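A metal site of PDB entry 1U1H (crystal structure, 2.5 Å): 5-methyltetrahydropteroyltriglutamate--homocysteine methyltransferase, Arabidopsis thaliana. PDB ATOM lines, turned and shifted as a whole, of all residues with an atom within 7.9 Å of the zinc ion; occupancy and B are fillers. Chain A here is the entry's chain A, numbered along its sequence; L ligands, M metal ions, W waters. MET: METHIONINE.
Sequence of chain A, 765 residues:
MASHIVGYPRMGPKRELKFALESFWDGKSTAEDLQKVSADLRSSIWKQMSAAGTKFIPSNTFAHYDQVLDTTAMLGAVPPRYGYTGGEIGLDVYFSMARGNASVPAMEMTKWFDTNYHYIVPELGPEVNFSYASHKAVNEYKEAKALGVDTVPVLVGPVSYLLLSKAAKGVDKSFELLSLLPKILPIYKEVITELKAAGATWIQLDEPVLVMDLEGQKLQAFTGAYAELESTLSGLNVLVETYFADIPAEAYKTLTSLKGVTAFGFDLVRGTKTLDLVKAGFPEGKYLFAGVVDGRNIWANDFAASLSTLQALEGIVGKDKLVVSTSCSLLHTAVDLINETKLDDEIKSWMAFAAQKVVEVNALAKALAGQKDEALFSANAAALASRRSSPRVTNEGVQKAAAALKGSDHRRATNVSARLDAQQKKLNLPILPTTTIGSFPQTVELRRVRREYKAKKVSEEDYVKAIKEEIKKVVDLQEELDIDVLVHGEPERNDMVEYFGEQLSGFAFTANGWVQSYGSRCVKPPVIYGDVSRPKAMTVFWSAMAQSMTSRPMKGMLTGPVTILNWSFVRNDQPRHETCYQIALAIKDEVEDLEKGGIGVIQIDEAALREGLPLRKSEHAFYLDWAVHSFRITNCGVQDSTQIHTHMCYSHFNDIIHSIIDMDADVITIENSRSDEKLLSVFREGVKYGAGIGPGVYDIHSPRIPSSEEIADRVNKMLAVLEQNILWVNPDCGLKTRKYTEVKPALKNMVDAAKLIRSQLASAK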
ATOM      1  N   ILE A 437       5.281  -3.199  -3.685  1.00  0.00           N
ATOM      2  CA  ILE A 437       5.375  -2.140  -2.695  1.00  0.00           C
ATOM      3  C   ILE A 437       5.530  -0.704  -3.202  1.00  0.00           C
ATOM      4  O   ILE A 437       5.329   0.237  -2.439  1.00  0.00           O
ATOM      5  CB  ILE A 437       6.485  -2.444  -1.706  1.00  0.00           C
ATOM      6  CG1 ILE A 437       6.291  -3.856  -1.151  1.00  0.00           C
ATOM      7  CG2 ILE A 437       6.473  -1.439  -0.562  1.00  0.00           C
ATOM      8  CD1 ILE A 437       4.912  -4.106  -0.588  1.00  0.00           C
ATOM      9  N   MET A 496      12.009   9.209  -0.888  1.00  0.00           N
ATOM     10  CA  MET A 496      10.745   9.025  -0.161  1.00  0.00           C
ATOM     11  C   MET A 496      10.264  10.271   0.544  1.00  0.00           C
ATOM     12  O   MET A 496       9.104  10.658   0.437  1.00  0.00           O
ATOM     13  CB  MET A 496      10.907   7.973   0.926  1.00  0.00           C
ATOM     14  CG  MET A 496      10.639   6.558   0.556  1.00  0.00           C
ATOM     15  SD  MET A 496      10.876   5.582   2.200  1.00  0.00           S
ATOM     16  CE  MET A 496       9.073   5.660   2.923  1.00  0.00           C
ATOM     17  N   ASP A 605       3.242   4.341   3.292  1.00  0.00           N
ATOM     18  CA  ASP A 605       4.293   3.560   3.938  1.00  0.00           C
ATOM     19  C   ASP A 605       4.995   4.311   5.058  1.00  0.00           C
ATOM     20  O   ASP A 605       5.406   5.468   4.907  1.00  0.00           O
ATOM     21  CB  ASP A 605       5.308   3.055   2.898  1.00  0.00           C
ATOM     22  CG  ASP A 605       5.736   4.126   1.913  1.00  0.00           C
ATOM     23  OD1 ASP A 605       5.908   5.280   2.348  1.00  0.00           O
ATOM     24  OD2 ASP A 605       5.917   3.820   0.707  1.00  0.00           O
ATOM     25  N   GLU A 606       5.089   3.648   6.207  1.00  0.00           N
ATOM     26  CA  GLU A 606       5.747   4.198   7.382  1.00  0.00           C
ATOM     27  C   GLU A 606       7.001   3.360   7.583  1.00  0.00           C
ATOM     28  O   GLU A 606       7.107   2.574   8.517  1.00  0.00           O
ATOM     29  CB  GLU A 606       4.835   4.109   8.599  1.00  0.00           C
ATOM     30  CG  GLU A 606       3.773   5.196   8.635  1.00  0.00           C
ATOM     31  CD  GLU A 606       4.376   6.555   8.934  1.00  0.00           C
ATOM     32  OE1 GLU A 606       5.477   6.844   8.419  1.00  0.00           O
ATOM     33  OE2 GLU A 606       3.757   7.338   9.665  1.00  0.00           O
ATOM     34  N   ALA A 607       7.943   3.553   6.668  1.00  0.00           N
ATOM     35  CA  ALA A 607       9.205   2.837   6.666  1.00  0.00           C
ATOM     36  C   ALA A 607       9.963   2.991   7.967  1.00  0.00           C
ATOM     37  O   ALA A 607      10.715   2.104   8.361  1.00  0.00           O
ATOM     38  CB  ALA A 607      10.078   3.337   5.509  1.00  0.00           C
ATOM     39  N   HIS A 647       2.708   0.358   4.524  1.00  0.00           N
ATOM     40  CA  HIS A 647       3.887  -0.488   4.386  1.00  0.00           C
ATOM     41  C   HIS A 647       4.915  -0.192   5.490  1.00  0.00           C
ATOM     42  O   HIS A 647       5.170   0.970   5.800  1.00  0.00           O
ATOM     43  CB  HIS A 647       4.520  -0.283   3.017  1.00  0.00           C
ATOM     44  CG  HIS A 647       5.833  -0.986   2.857  1.00  0.00           C
ATOM     45  ND1 HIS A 647       5.961  -2.349   2.968  1.00  0.00           N
ATOM     46  CD2 HIS A 647       7.081  -0.501   2.654  1.00  0.00           C
ATOM     47  CE1 HIS A 647       7.231  -2.683   2.826  1.00  0.00           C
ATOM     48  NE2 HIS A 647       7.930  -1.583   2.633  1.00  0.00           N
ATOM     49  N   MET A 648       5.511  -1.236   6.060  1.00  0.00           N
ATOM     50  CA  MET A 648       6.509  -1.050   7.125  1.00  0.00           C
ATOM     51  C   MET A 648       7.725  -1.959   7.009  1.00  0.00           C
ATOM     52  O   MET A 648       7.627  -3.175   7.123  1.00  0.00           O
ATOM     53  CB  MET A 648       5.855  -1.246   8.493  1.00  0.00           C
ATOM     54  CG  MET A 648       4.776  -0.227   8.790  1.00  0.00           C
ATOM     55  SD  MET A 648       3.798  -0.634  10.388  1.00  0.00           S
ATOM     56  CE  MET A 648       2.712  -2.065   9.681  1.00  0.00           C
ATOM     57  N   CYS A 649       8.886  -1.340   6.816  1.00  0.00           N
ATOM     58  CA  CYS A 649      10.140  -2.069   6.675  1.00  0.00           C
ATOM     59  C   CYS A 649      10.613  -2.748   7.954  1.00  0.00           C
ATOM     60  O   CYS A 649      11.618  -2.347   8.521  1.00  0.00           O
ATOM     61  CB  CYS A 649      11.213  -1.117   6.169  1.00  0.00           C
ATOM     62  SG  CYS A 649      10.665  -0.046   4.829  1.00  0.00           S
ATOM     63  N   TYR A 650       9.905  -3.786   8.396  1.00  0.00           N
ATOM     64  CA  TYR A 650      10.273  -4.506   9.615  1.00  0.00           C
ATOM     65  C   TYR A 650       9.751  -5.952   9.555  1.00  0.00           C
ATOM     66  O   TYR A 650       8.837  -6.253   8.803  1.00  0.00           O
ATOM     67  CB  TYR A 650       9.659  -3.827  10.847  1.00  0.00           C
ATOM     68  CG  TYR A 650      10.076  -2.385  11.052  1.00  0.00           C
ATOM     69  CD1 TYR A 650      11.357  -2.058  11.509  1.00  0.00           C
ATOM     70  CD2 TYR A 650       9.184  -1.342  10.802  1.00  0.00           C
ATOM     71  CE1 TYR A 650      11.728  -0.735  11.713  1.00  0.00           C
ATOM     72  CE2 TYR A 650       9.542  -0.015  11.010  1.00  0.00           C
ATOM     73  CZ  TYR A 650      10.818   0.282  11.462  1.00  0.00           C
ATOM     74  OH  TYR A 650      11.172   1.603  11.691  1.00  0.00           O
ATOM     75  N   THR A 669       1.496  -4.341   4.821  1.00  0.00           N
ATOM     76  CA  THR A 669       2.503  -5.210   4.233  1.00  0.00           C
ATOM     77  C   THR A 669       3.794  -5.006   5.025  1.00  0.00           C
ATOM     78  O   THR A 669       4.239  -3.871   5.219  1.00  0.00           O
ATOM     79  CB  THR A 669       2.693  -4.855   2.749  1.00  0.00           C
ATOM     80  OG1 THR A 669       3.546  -5.831   2.149  1.00  0.00           O
ATOM     81  CG2 THR A 669       3.308  -3.494   2.601  1.00  0.00           C
ATOM     82  N   ILE A 670       4.373  -6.098   5.497  1.00  0.00           N
ATOM     83  CA  ILE A 670       5.597  -6.024   6.284  1.00  0.00           C
ATOM     84  C   ILE A 670       6.734  -6.821   5.619  1.00  0.00           C
ATOM     85  O   ILE A 670       6.558  -7.375   4.534  1.00  0.00           O
ATOM     86  CB  ILE A 670       5.380  -6.601   7.702  1.00  0.00           C
ATOM     87  CG1 ILE A 670       5.081  -8.103   7.594  1.00  0.00           C
ATOM     88  CG2 ILE A 670       4.236  -5.875   8.406  1.00  0.00           C
ATOM     89  CD1 ILE A 670       4.979  -8.814   8.935  1.00  0.00           C
ATOM     90  N   GLU A 671       7.880  -6.875   6.287  1.00  0.00           N
ATOM     91  CA  GLU A 671       9.047  -7.614   5.801  1.00  0.00           C
ATOM     92  C   GLU A 671       8.974  -9.057   6.278  1.00  0.00           C
ATOM     93  O   GLU A 671       8.676  -9.316   7.445  1.00  0.00           O
ATOM     94  CB  GLU A 671      10.325  -6.986   6.310  1.00  0.00           C
ATOM     95  CG  GLU A 671      10.891  -5.938   5.391  1.00  0.00           C
ATOM     96  CD  GLU A 671      12.142  -5.312   5.942  1.00  0.00           C
ATOM     97  OE1 GLU A 671      12.947  -6.055   6.536  1.00  0.00           O
ATOM     98  OE2 GLU A 671      12.326  -4.097   5.752  1.00  0.00           O
ATOM     99  N   ILE A 700      14.169  -8.360  -1.624  1.00  0.00           N
ATOM    100  CA  ILE A 700      14.632  -7.398  -2.617  1.00  0.00           C
ATOM    101  C   ILE A 700      16.074  -6.927  -2.429  1.00  0.00           C
ATOM    102  O   ILE A 700      16.597  -6.162  -3.237  1.00  0.00           O
ATOM    103  CB  ILE A 700      13.755  -6.136  -2.627  1.00  0.00           C
ATOM    104  CG1 ILE A 700      13.808  -5.454  -1.256  1.00  0.00           C
ATOM    105  CG2 ILE A 700      12.326  -6.504  -3.004  1.00  0.00           C
ATOM    106  CD1 ILE A 700      13.716  -3.948  -1.322  1.00  0.00           C
ATOM    107  N   HIS A 701      16.719  -7.361  -1.358  1.00  0.00           N
ATOM    108  CA  HIS A 701      18.093  -6.951  -1.111  1.00  0.00           C
ATOM    109  C   HIS A 701      19.113  -7.905  -1.707  1.00  0.00           C
ATOM    110  O   HIS A 701      20.306  -7.627  -1.707  1.00  0.00           O
ATOM    111  CB  HIS A 701      18.324  -6.778   0.395  1.00  0.00           C
ATOM    112  CG  HIS A 701      17.576  -5.628   0.990  1.00  0.00           C
ATOM    113  ND1 HIS A 701      16.647  -5.782   2.000  1.00  0.00           N
ATOM    114  CD2 HIS A 701      17.623  -4.312   0.717  1.00  0.00           C
ATOM    115  CE1 HIS A 701      16.148  -4.601   2.317  1.00  0.00           C
ATOM    116  NE2 HIS A 701      16.724  -3.690   1.553  1.00  0.00           N
ATOM    117  N   PRO A 731       6.264  -8.505  -2.564  1.00  0.00           N
ATOM    118  CA  PRO A 731       7.684  -8.538  -2.181  1.00  0.00           C
ATOM    119  C   PRO A 731       7.972  -7.984  -0.783  1.00  0.00           C
ATOM    120  O   PRO A 731       7.062  -7.556  -0.074  1.00  0.00           O
ATOM    121  CB  PRO A 731       8.360  -7.705  -3.269  1.00  0.00           C
ATOM    122  CG  PRO A 731       7.390  -7.783  -4.429  1.00  0.00           C
ATOM    123  CD  PRO A 731       6.064  -7.649  -3.736  1.00  0.00           C
ATOM    124  N   ASP A 732       9.243  -7.985  -0.412  1.00  0.00           N
ATOM    125  CA  ASP A 732       9.712  -7.495   0.886  1.00  0.00           C
ATOM    126  C   ASP A 732       9.671  -5.980   0.974  1.00  0.00           C
ATOM    127  O   ASP A 732       9.460  -5.416   2.044  1.00  0.00           O
ATOM    128  CB  ASP A 732      11.156  -7.940   1.140  1.00  0.00           C
ATOM    129  CG  ASP A 732      11.257  -9.119   2.083  1.00  0.00           C
ATOM    130  OD1 ASP A 732      10.233  -9.477   2.706  1.00  0.00           O
ATOM    131  OD2 ASP A 732      12.372  -9.673   2.221  1.00  0.00           O
ATOM    132  N   CYS A 733       9.910  -5.325  -0.160  1.00  0.00           N
ATOM    133  CA  CYS A 733       9.907  -3.873  -0.231  1.00  0.00           C
ATOM    134  C   CYS A 733       9.916  -3.439  -1.686  1.00  0.00           C
ATOM    135  O   CYS A 733       9.592  -4.234  -2.571  1.00  0.00           O
ATOM    136  CB  CYS A 733      11.128  -3.298   0.489  1.00  0.00           C
ATOM    137  SG  CYS A 733      11.061  -1.492   0.745  1.00  0.00           S
ATOM    138  N   GLY A 734      10.280  -2.190  -1.923  1.00  0.00           N
ATOM    139  CA  GLY A 734      10.335  -1.650  -3.281  1.00  0.00           C
ATOM    140  C   GLY A 734      11.338  -2.403  -4.128  1.00  0.00           C
ATOM    141  O   GLY A 734      12.045  -3.285  -3.631  1.00  0.00           O
HETATM  142  N   MET L   1       6.893   2.774  -1.782  1.00  0.00           N
HETATM  143  CA  MET L   1       8.363   3.025  -1.793  1.00  0.00           C
HETATM  144  C   MET L   1       9.084   1.920  -2.560  1.00  0.00           C
HETATM  145  O   MET L   1       8.415   0.983  -3.033  1.00  0.00           O
HETATM  146  CB  MET L   1       8.892   3.088  -0.362  1.00  0.00           C
HETATM  147  CG  MET L   1       8.947   1.751   0.350  1.00  0.00           C
HETATM  148  SD  MET L   1       9.438   1.904   2.086  1.00  0.00           S
HETATM  149  CE  MET L   1      11.229   2.156   1.963  1.00  0.00           C
HETATM  150  OXT MET L   1      10.323   2.017  -2.673  1.00  0.00           O
HETATM  151 ZN    ZN M   1      10.083  -1.511   2.990  1.00  0.00          ZN
HETATM  152  O   HOH W   1      10.340  -3.637   3.823  1.00  0.00           O
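A sulfur (SD) of the ligand lies close to the side-chain sulfur of Cys 649. The backbone carbonyl oxygen of Ile 437 is in hydrogen-bond range of a nitrogen (N) of the ligand (3.1 Å). A nitrogen (N) of the ligand is in salt-bridge range of the side-chain carboxylate (OD2) of Asp 605 (2.9 Å).
A ring nitrogen (ND1) of His 647 lies close to the backbone carbonyl oxygen (O) of Thr 669. The backbone carbonyl oxygen of His 647 is in hydrogen-bond range of the backbone NH of Glu 606, 2.7 Å away.
Three residues have an atom within 4 Å of the zinc ion: His 647, Cys 649 and Cys 733. The nearest printed residue that does not touch the zinc ion is Asp 732 (4.1 Å).
The zinc ion is bound by NE2 of His 647 (2.2 Å), water W1 (2.3 Å), SG of Cys 649 (2.4 Å) and SG of Cys 733 (2.4 Å). The zinc ion has four donor atoms within binding distance.
Water W1 bridges O of Asp 732 and OE2 of Glu 671.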
